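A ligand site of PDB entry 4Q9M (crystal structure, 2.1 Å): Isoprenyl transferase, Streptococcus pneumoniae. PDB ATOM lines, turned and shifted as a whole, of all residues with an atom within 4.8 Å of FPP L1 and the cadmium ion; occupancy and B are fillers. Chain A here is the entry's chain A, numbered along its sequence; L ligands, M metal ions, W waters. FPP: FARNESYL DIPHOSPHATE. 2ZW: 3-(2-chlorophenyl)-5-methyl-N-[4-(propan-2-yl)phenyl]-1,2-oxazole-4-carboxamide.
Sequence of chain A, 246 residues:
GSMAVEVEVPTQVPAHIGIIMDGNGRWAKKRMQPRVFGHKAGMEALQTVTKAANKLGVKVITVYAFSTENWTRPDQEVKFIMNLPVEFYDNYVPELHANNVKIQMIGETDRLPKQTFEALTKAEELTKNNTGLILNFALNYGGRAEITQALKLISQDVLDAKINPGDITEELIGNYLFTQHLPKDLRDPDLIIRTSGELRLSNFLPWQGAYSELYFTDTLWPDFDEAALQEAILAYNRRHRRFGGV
Residues that only touch FPP L1: Ala 65 (3.2 Å), Met 21 (3.4 Å), His 39 (3.5 Å), Ile 81 (3.6 Å), Leu 46 (3.7 Å), Gly 42 (3.7 Å), Phe 137 (3.7 Å) and Met 43 (3.8 Å).
Hydrophobic or aromatic side chains that line FPP L1: Met 21, His 39, Leu 46, Ala 65, Ile 81 and Phe 137.
The nearest printed residue that does not touch FPP L1 is Asn 70 (4.2 Å).
The side-chain carboxylate (OD1) of Asp 22 sits close to the guanidinium group (NH1) of Arg 26 (3.7 Å).
NH1 of Arg 73 is in salt-bridge range of OE1 of Glu 77, at 2.9 Å.
A ring nitrogen (ND1) of His 39 lies within hydrogen-bond range of the side-chain amide oxygen (OD1) of Asn 24, at 3.1 Å.
NH2 of Arg 35 is in salt-bridge range of OE2 of Glu 77 (2.8 Å).
The side-chain carboxylate of Glu 77 is in hydrogen-bond range of a ring nitrogen (NE2) of His 39 (2.8 Å).
The nearest printed residue that does not touch the cadmium ion is Arg 26 (4.01 Å).
The cadmium ion is bound by an oxygen (O2A) of FPP L1 (2.2 Å), an oxygen (O2B) of FPP L1 (2.2 Å), the side-chain carboxylate of Asp 22 (2.3 Å), water W4 (2.4 Å), water W2 (2.4 Å) and water W1 (2.5 Å).
The cadmium ion has six donor atoms within binding distance.
The backbone NH of Arg 26 lies within hydrogen-bond range of an oxygen (O1B) of FPP L1.
The guanidinium group (NE) of Arg 26 is in salt-bridge range of an oxygen (O1B) of FPP L1 (2.8 Å).
The guanidinium group of Arg 73 is in salt-bridge range of an oxygen (O1A) of FPP L1 (2.9 Å).
N of Gly 25 lies within hydrogen-bond range of O3A of FPP L1 (3.0 Å).
An oxygen (O3A) of FPP L1 is in hydrogen-bond range of the backbone NH (N) of Asn 24.
The guanidinium group of Arg 35 is in salt-bridge range of an oxygen (O3B) of FPP L1 (3.4 Å).
An oxygen (O3A) of FPP L1 sits at hydrogen-bond distance from the backbone NH (N) of Gly 23 (3.5 Å).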
ATOM      1  N   MET A  21      32.673  22.023   6.025  1.00  0.00           N
ATOM      2  CA  MET A  21      31.810  23.022   6.629  1.00  0.00           C
ATOM      3  C   MET A  21      32.329  23.302   8.023  1.00  0.00           C
ATOM      4  O   MET A  21      32.576  22.363   8.794  1.00  0.00           O
ATOM      5  CB  MET A  21      30.365  22.505   6.698  1.00  0.00           C
ATOM      6  CG  MET A  21      29.797  22.091   5.355  1.00  0.00           C
ATOM      7  SD  MET A  21      28.168  21.287   5.536  1.00  0.00           S
ATOM      8  CE  MET A  21      28.617  19.839   6.605  1.00  0.00           C
ATOM      9  N   ASP A  22      32.594  24.567   8.325  1.00  0.00           N
ATOM     10  CA  ASP A  22      33.112  24.925   9.639  1.00  0.00           C
ATOM     11  C   ASP A  22      32.606  26.277  10.079  1.00  0.00           C
ATOM     12  O   ASP A  22      32.334  27.123   9.232  1.00  0.00           O
ATOM     13  CB  ASP A  22      34.657  24.897   9.622  1.00  0.00           C
ATOM     14  CG  ASP A  22      35.309  24.586  10.955  1.00  0.00           C
ATOM     15  OD1 ASP A  22      34.572  24.408  11.966  1.00  0.00           O
ATOM     16  OD2 ASP A  22      36.528  24.416  10.983  1.00  0.00           O
ATOM     17  N   GLY A  23      32.515  26.475  11.390  1.00  0.00           N
ATOM     18  CA  GLY A  23      32.096  27.755  11.972  1.00  0.00           C
ATOM     19  C   GLY A  23      30.635  27.855  12.374  1.00  0.00           C
ATOM     20  O   GLY A  23      30.162  28.956  12.646  1.00  0.00           O
ATOM     21  N   ASN A  24      29.909  26.719  12.423  1.00  0.00           N
ATOM     22  CA  ASN A  24      28.498  26.696  12.816  1.00  0.00           C
ATOM     23  C   ASN A  24      28.300  27.179  14.254  1.00  0.00           C
ATOM     24  O   ASN A  24      27.367  27.937  14.519  1.00  0.00           O
ATOM     25  CB  ASN A  24      27.879  25.289  12.667  1.00  0.00           C
ATOM     26  CG  ASN A  24      27.783  24.717  11.277  1.00  0.00           C
ATOM     27  OD1 ASN A  24      27.420  23.550  11.099  1.00  0.00           O
ATOM     28  ND2 ASN A  24      28.093  25.494  10.250  1.00  0.00           N
ATOM     29  N   GLY A  25      29.186  26.763  15.163  1.00  0.00           N
ATOM     30  CA  GLY A  25      29.124  27.147  16.570  1.00  0.00           C
ATOM     31  C   GLY A  25      29.411  28.618  16.788  1.00  0.00           C
ATOM     32  O   GLY A  25      28.651  29.294  17.482  1.00  0.00           O
ATOM     33  N   ARG A  26      30.472  29.150  16.145  1.00  0.00           N
ATOM     34  CA  ARG A  26      30.831  30.569  16.227  1.00  0.00           C
ATOM     35  C   ARG A  26      29.728  31.418  15.621  1.00  0.00           C
ATOM     36  O   ARG A  26      29.391  32.461  16.170  1.00  0.00           O
ATOM     37  CB  ARG A  26      32.156  30.847  15.496  1.00  0.00           C
ATOM     38  CG  ARG A  26      33.380  30.578  16.355  1.00  0.00           C
ATOM     39  CD  ARG A  26      34.604  30.452  15.477  1.00  0.00           C
ATOM     40  NE  ARG A  26      34.707  29.108  14.905  1.00  0.00           N
ATOM     41  CZ  ARG A  26      35.664  28.716  14.070  1.00  0.00           C
ATOM     42  NH1 ARG A  26      35.691  27.474  13.625  1.00  0.00           N
ATOM     43  NH2 ARG A  26      36.606  29.567  13.689  1.00  0.00           N
ATOM     44  N   ARG A  35      25.150  25.950  19.634  1.00  0.00           N
ATOM     45  CA  ARG A  35      25.783  25.396  18.438  1.00  0.00           C
ATOM     46  C   ARG A  35      24.777  24.721  17.465  1.00  0.00           C
ATOM     47  O   ARG A  35      24.885  24.912  16.257  1.00  0.00           O
ATOM     48  CB  ARG A  35      26.905  24.440  18.851  1.00  0.00           C
ATOM     49  CG  ARG A  35      27.739  23.878  17.716  1.00  0.00           C
ATOM     50  CD  ARG A  35      29.211  23.760  18.081  1.00  0.00           C
ATOM     51  NE  ARG A  35      29.519  22.571  18.872  1.00  0.00           N
ATOM     52  CZ  ARG A  35      30.727  22.032  18.988  1.00  0.00           C
ATOM     53  NH1 ARG A  35      31.761  22.547  18.345  1.00  0.00           N
ATOM     54  NH2 ARG A  35      30.909  20.955  19.749  1.00  0.00           N
ATOM     55  N   HIS A  39      23.915  24.466  13.309  1.00  0.00           N
ATOM     56  CA  HIS A  39      23.878  23.260  12.453  1.00  0.00           C
ATOM     57  C   HIS A  39      22.658  23.279  11.534  1.00  0.00           C
ATOM     58  O   HIS A  39      22.793  22.935  10.361  1.00  0.00           O
ATOM     59  CB  HIS A  39      23.925  21.967  13.285  1.00  0.00           C
ATOM     60  CG  HIS A  39      25.170  21.806  14.119  1.00  0.00           C
ATOM     61  ND1 HIS A  39      26.374  22.391  13.757  1.00  0.00           N
ATOM     62  CD2 HIS A  39      25.349  21.104  15.259  1.00  0.00           C
ATOM     63  CE1 HIS A  39      27.226  22.056  14.702  1.00  0.00           C
ATOM     64  NE2 HIS A  39      26.677  21.260  15.611  1.00  0.00           N
ATOM     65  N   GLY A  42      23.320  25.661   8.911  1.00  0.00           N
ATOM     66  CA  GLY A  42      24.285  24.974   8.047  1.00  0.00           C
ATOM     67  C   GLY A  42      23.593  24.154   6.956  1.00  0.00           C
ATOM     68  O   GLY A  42      24.096  24.078   5.839  1.00  0.00           O
ATOM     69  N   MET A  43      22.414  23.567   7.260  1.00  0.00           N
ATOM     70  CA  MET A  43      21.620  22.802   6.294  1.00  0.00           C
ATOM     71  C   MET A  43      21.042  23.722   5.233  1.00  0.00           C
ATOM     72  O   MET A  43      21.008  23.354   4.073  1.00  0.00           O
ATOM     73  CB  MET A  43      20.464  22.039   6.977  1.00  0.00           C
ATOM     74  CG  MET A  43      20.918  20.907   7.881  1.00  0.00           C
ATOM     75  SD  MET A  43      19.483  20.193   8.716  1.00  0.00           S
ATOM     76  CE  MET A  43      18.912  19.032   7.489  1.00  0.00           C
ATOM     77  N   LEU A  46      23.813  24.639   2.926  1.00  0.00           N
ATOM     78  CA  LEU A  46      24.117  23.520   2.018  1.00  0.00           C
ATOM     79  C   LEU A  46      23.087  23.431   0.877  1.00  0.00           C
ATOM     80  O   LEU A  46      23.480  23.227  -0.274  1.00  0.00           O
ATOM     81  CB  LEU A  46      24.252  22.179   2.776  1.00  0.00           C
ATOM     82  CG  LEU A  46      24.637  20.963   1.899  1.00  0.00           C
ATOM     83  CD1 LEU A  46      25.960  21.202   1.155  1.00  0.00           C
ATOM     84  CD2 LEU A  46      24.686  19.678   2.703  1.00  0.00           C
ATOM     85  N   VAL A  63      30.547  16.638   0.806  1.00  0.00           N
ATOM     86  CA  VAL A  63      30.516  17.419   2.039  1.00  0.00           C
ATOM     87  C   VAL A  63      30.951  16.573   3.212  1.00  0.00           C
ATOM     88  O   VAL A  63      30.509  15.439   3.341  1.00  0.00           O
ATOM     89  CB  VAL A  63      29.136  18.113   2.205  1.00  0.00           C
ATOM     90  CG1 VAL A  63      28.016  17.149   2.586  1.00  0.00           C
ATOM     91  CG2 VAL A  63      29.234  19.257   3.166  1.00  0.00           C
ATOM     92  N   ALA A  65      30.111  15.833   6.232  1.00  0.00           N
ATOM     93  CA  ALA A  65      28.972  15.916   7.149  1.00  0.00           C
ATOM     94  C   ALA A  65      29.249  15.396   8.554  1.00  0.00           C
ATOM     95  O   ALA A  65      28.776  15.998   9.513  1.00  0.00           O
ATOM     96  CB  ALA A  65      27.767  15.204   6.560  1.00  0.00           C
ATOM     97  N   PHE A  66      29.965  14.269   8.691  1.00  0.00           N
ATOM     98  CA  PHE A  66      30.243  13.741  10.034  1.00  0.00           C
ATOM     99  C   PHE A  66      31.498  12.907  10.022  1.00  0.00           C
ATOM    100  O   PHE A  66      31.540  11.837   9.407  1.00  0.00           O
ATOM    101  CB  PHE A  66      29.038  12.939  10.605  1.00  0.00           C
ATOM    102  CG  PHE A  66      28.995  12.887  12.120  1.00  0.00           C
ATOM    103  CD1 PHE A  66      28.369  13.902  12.855  1.00  0.00           C
ATOM    104  CD2 PHE A  66      29.525  11.804  12.816  1.00  0.00           C
ATOM    105  CE1 PHE A  66      28.300  13.845  14.262  1.00  0.00           C
ATOM    106  CE2 PHE A  66      29.441  11.734  14.218  1.00  0.00           C
ATOM    107  CZ  PHE A  66      28.835  12.754  14.926  1.00  0.00           C
ATOM    108  N   ASN A  70      33.889  13.485  15.199  1.00  0.00           N
ATOM    109  CA  ASN A  70      32.677  14.205  15.648  1.00  0.00           C
ATOM    110  C   ASN A  70      31.862  13.433  16.703  1.00  0.00           C
ATOM    111  O   ASN A  70      31.068  14.051  17.406  1.00  0.00           O
ATOM    112  CB  ASN A  70      31.808  14.612  14.457  1.00  0.00           C
ATOM    113  CG  ASN A  70      32.418  15.650  13.530  1.00  0.00           C
ATOM    114  OD1 ASN A  70      32.073  15.704  12.349  1.00  0.00           O
ATOM    115  ND2 ASN A  70      33.338  16.479  14.008  1.00  0.00           N
ATOM    116  N   ARG A  73      31.894  14.725  20.423  1.00  0.00           N
ATOM    117  CA  ARG A  73      31.122  15.924  20.814  1.00  0.00           C
ATOM    118  C   ARG A  73      30.140  15.552  21.936  1.00  0.00           C
ATOM    119  O   ARG A  73      29.874  14.357  22.100  1.00  0.00           O
ATOM    120  CB  ARG A  73      30.381  16.483  19.584  1.00  0.00           C
ATOM    121  CG  ARG A  73      31.316  17.276  18.689  1.00  0.00           C
ATOM    122  CD  ARG A  73      30.643  17.817  17.438  1.00  0.00           C
ATOM    123  NE  ARG A  73      31.645  18.471  16.603  1.00  0.00           N
ATOM    124  CZ  ARG A  73      31.530  19.679  16.051  1.00  0.00           C
ATOM    125  NH1 ARG A  73      30.409  20.370  16.189  1.00  0.00           N
ATOM    126  NH2 ARG A  73      32.512  20.177  15.323  1.00  0.00           N
ATOM    127  N   GLU A  77      24.443  16.943  21.618  1.00  0.00           N
ATOM    128  CA  GLU A  77      24.730  17.517  20.298  1.00  0.00           C
ATOM    129  C   GLU A  77      24.787  16.426  19.211  1.00  0.00           C
ATOM    130  O   GLU A  77      24.202  16.609  18.143  1.00  0.00           O
ATOM    131  CB  GLU A  77      26.040  18.327  20.333  1.00  0.00           C
ATOM    132  CG  GLU A  77      26.322  19.042  19.010  1.00  0.00           C
ATOM    133  CD  GLU A  77      27.674  19.726  18.915  1.00  0.00           C
ATOM    134  OE1 GLU A  77      28.042  20.148  17.802  1.00  0.00           O
ATOM    135  OE2 GLU A  77      28.375  19.824  19.953  1.00  0.00           O
ATOM    136  N   ILE A  81      22.297  16.171  15.953  1.00  0.00           N
ATOM    137  CA  ILE A  81      22.867  16.088  14.604  1.00  0.00           C
ATOM    138  C   ILE A  81      22.320  14.902  13.831  1.00  0.00           C
ATOM    139  O   ILE A  81      21.886  15.061  12.689  1.00  0.00           O
ATOM    140  CB  ILE A  81      24.428  16.070  14.673  1.00  0.00           C
ATOM    141  CG1 ILE A  81      24.993  17.416  15.154  1.00  0.00           C
ATOM    142  CG2 ILE A  81      25.046  15.659  13.311  1.00  0.00           C
ATOM    143  CD1 ILE A  81      26.548  17.373  15.527  1.00  0.00           C
ATOM    144  N   LEU A  84      18.819  15.317  12.458  1.00  0.00           N
ATOM    145  CA  LEU A  84      18.552  16.349  11.430  1.00  0.00           C
ATOM    146  C   LEU A  84      17.999  15.800  10.123  1.00  0.00           C
ATOM    147  O   LEU A  84      16.946  16.284   9.701  1.00  0.00           O
ATOM    148  CB  LEU A  84      19.756  17.252  11.172  1.00  0.00           C
ATOM    149  CG  LEU A  84      20.185  18.162  12.347  1.00  0.00           C
ATOM    150  CD1 LEU A  84      21.613  18.742  12.087  1.00  0.00           C
ATOM    151  CD2 LEU A  84      19.169  19.274  12.577  1.00  0.00           C
ATOM    152  N   PHE A 137      27.389  12.880   0.746  1.00  0.00           N
ATOM    153  CA  PHE A 137      27.598  13.108   2.176  1.00  0.00           C
ATOM    154  C   PHE A 137      28.680  12.164   2.737  1.00  0.00           C
ATOM    155  O   PHE A 137      28.476  10.945   2.722  1.00  0.00           O
ATOM    156  CB  PHE A 137      26.270  12.881   2.938  1.00  0.00           C
ATOM    157  CG  PHE A 137      25.210  13.930   2.693  1.00  0.00           C
ATOM    158  CD1 PHE A 137      24.316  13.793   1.617  1.00  0.00           C
ATOM    159  CD2 PHE A 137      25.103  15.044   3.514  1.00  0.00           C
ATOM    160  CE1 PHE A 137      23.345  14.781   1.369  1.00  0.00           C
ATOM    161  CE2 PHE A 137      24.112  16.017   3.282  1.00  0.00           C
ATOM    162  CZ  PHE A 137      23.233  15.873   2.221  1.00  0.00           C
HETATM  163  C1  FPP L   1      30.918  22.682  11.742  1.00  0.00           C
HETATM  164  O1  FPP L   1      30.877  23.709  12.722  1.00  0.00           O
HETATM  165  C2  FPP L   1      30.177  21.508  12.260  1.00  0.00           C
HETATM  166  C3  FPP L   1      30.606  20.245  12.248  1.00  0.00           C
HETATM  167  C4  FPP L   1      31.966  19.825  11.747  1.00  0.00           C
HETATM  168  C5  FPP L   1      29.718  19.130  12.740  1.00  0.00           C
HETATM  169  C6  FPP L   1      28.939  18.405  11.602  1.00  0.00           C
HETATM  170  C7  FPP L   1      28.065  19.340  10.784  1.00  0.00           C
HETATM  171  C8  FPP L   1      26.777  19.631  10.971  1.00  0.00           C
HETATM  172  C10 FPP L   1      25.929  19.008  12.037  1.00  0.00           C
HETATM  173  C9  FPP L   1      26.093  20.669  10.113  1.00  0.00           C
HETATM  174  C11 FPP L   1      24.789  20.198   9.402  1.00  0.00           C
HETATM  175  C12 FPP L   1      25.084  19.135   8.376  1.00  0.00           C
HETATM  176  C13 FPP L   1      25.008  19.187   7.058  1.00  0.00           C
HETATM  177  C14 FPP L   1      25.364  18.010   6.196  1.00  0.00           C
HETATM  178  C15 FPP L   1      24.556  20.396   6.295  1.00  0.00           C
HETATM  179  PA  FPP L   1      31.474  23.658  14.217  1.00  0.00           P
HETATM  180  O1A FPP L   1      30.501  23.106  15.204  1.00  0.00           O
HETATM  181  O2A FPP L   1      32.757  22.936  14.300  1.00  0.00           O
HETATM  182  O3A FPP L   1      31.720  25.213  14.516  1.00  0.00           O
HETATM  183  PB  FPP L   1      32.791  25.999  15.381  1.00  0.00           P
HETATM  184  O1B FPP L   1      32.532  27.433  15.313  1.00  0.00           O
HETATM  185  O2B FPP L   1      34.170  25.546  14.879  1.00  0.00           O
HETATM  186  O3B FPP L   1      32.609  25.436  16.774  1.00  0.00           O
HETATM  187  CP3 2ZW L   2      25.492  14.798   9.965  1.00  0.00           C
HETATM  188  CP1 2ZW L   2      23.982  14.562   9.988  1.00  0.00           C
HETATM  189  CP2 2ZW L   2      23.692  13.084  10.249  1.00  0.00           C
HETATM  190  C44 2ZW L   2      23.321  15.098   8.721  1.00  0.00           C
HETATM  191  C45 2ZW L   2      22.825  16.401   8.695  1.00  0.00           C
HETATM  192  C46 2ZW L   2      22.182  16.906   7.570  1.00  0.00           C
HETATM  193  C43 2ZW L   2      23.183  14.319   7.584  1.00  0.00           C
HETATM  194  C42 2ZW L   2      22.556  14.811   6.449  1.00  0.00           C
HETATM  195  C41 2ZW L   2      22.042  16.113   6.435  1.00  0.00           C
HETATM  196  N3  2ZW L   2      21.373  16.530   5.259  1.00  0.00           N
HETATM  197  C3  2ZW L   2      21.151  17.809   4.770  1.00  0.00           C
HETATM  198  O3  2ZW L   2      21.679  18.811   5.233  1.00  0.00           O
HETATM  199  C25 2ZW L   2      20.291  17.900   3.558  1.00  0.00           C
HETATM  200  C24 2ZW L   2      20.171  18.987   2.762  1.00  0.00           C
HETATM  201  CM  2ZW L   2      20.526  20.424   2.886  1.00  0.00           C
HETATM  202  O23 2ZW L   2      19.662  18.613   1.577  1.00  0.00           O
HETATM  203  N22 2ZW L   2      19.432  17.201   1.627  1.00  0.00           N
HETATM  204  C21 2ZW L   2      19.788  16.812   2.834  1.00  0.00           C
HETATM  205  C11 2ZW L   2      19.248  15.477   3.197  1.00  0.00           C
HETATM  206  C12 2ZW L   2      18.309  15.246   4.194  1.00  0.00           C
HETATM  207 CL   2ZW L   2      17.558  16.573   5.034  1.00  0.00          CL
HETATM  208  C13 2ZW L   2      17.864  13.964   4.478  1.00  0.00           C
HETATM  209  C14 2ZW L   2      18.366  12.889   3.765  1.00  0.00           C
HETATM  210  C15 2ZW L   2      19.265  13.114   2.740  1.00  0.00           C
HETATM  211  C16 2ZW L   2      19.653  14.397   2.414  1.00  0.00           C
HETATM  212 CD    CD M   1      34.835  23.594  14.141  1.00  0.00          CD
HETATM  213  O   HOH W   1      35.526  22.505  16.267  1.00  0.00           O
HETATM  214  O   HOH W   2      35.578  21.558  12.999  1.00  0.00           O
HETATM  215  O   HOH W   3      32.000  26.871  18.882  1.00  0.00           O
HETATM  216  O   HOH W   4      37.131  24.232  13.580  1.00  0.00           O
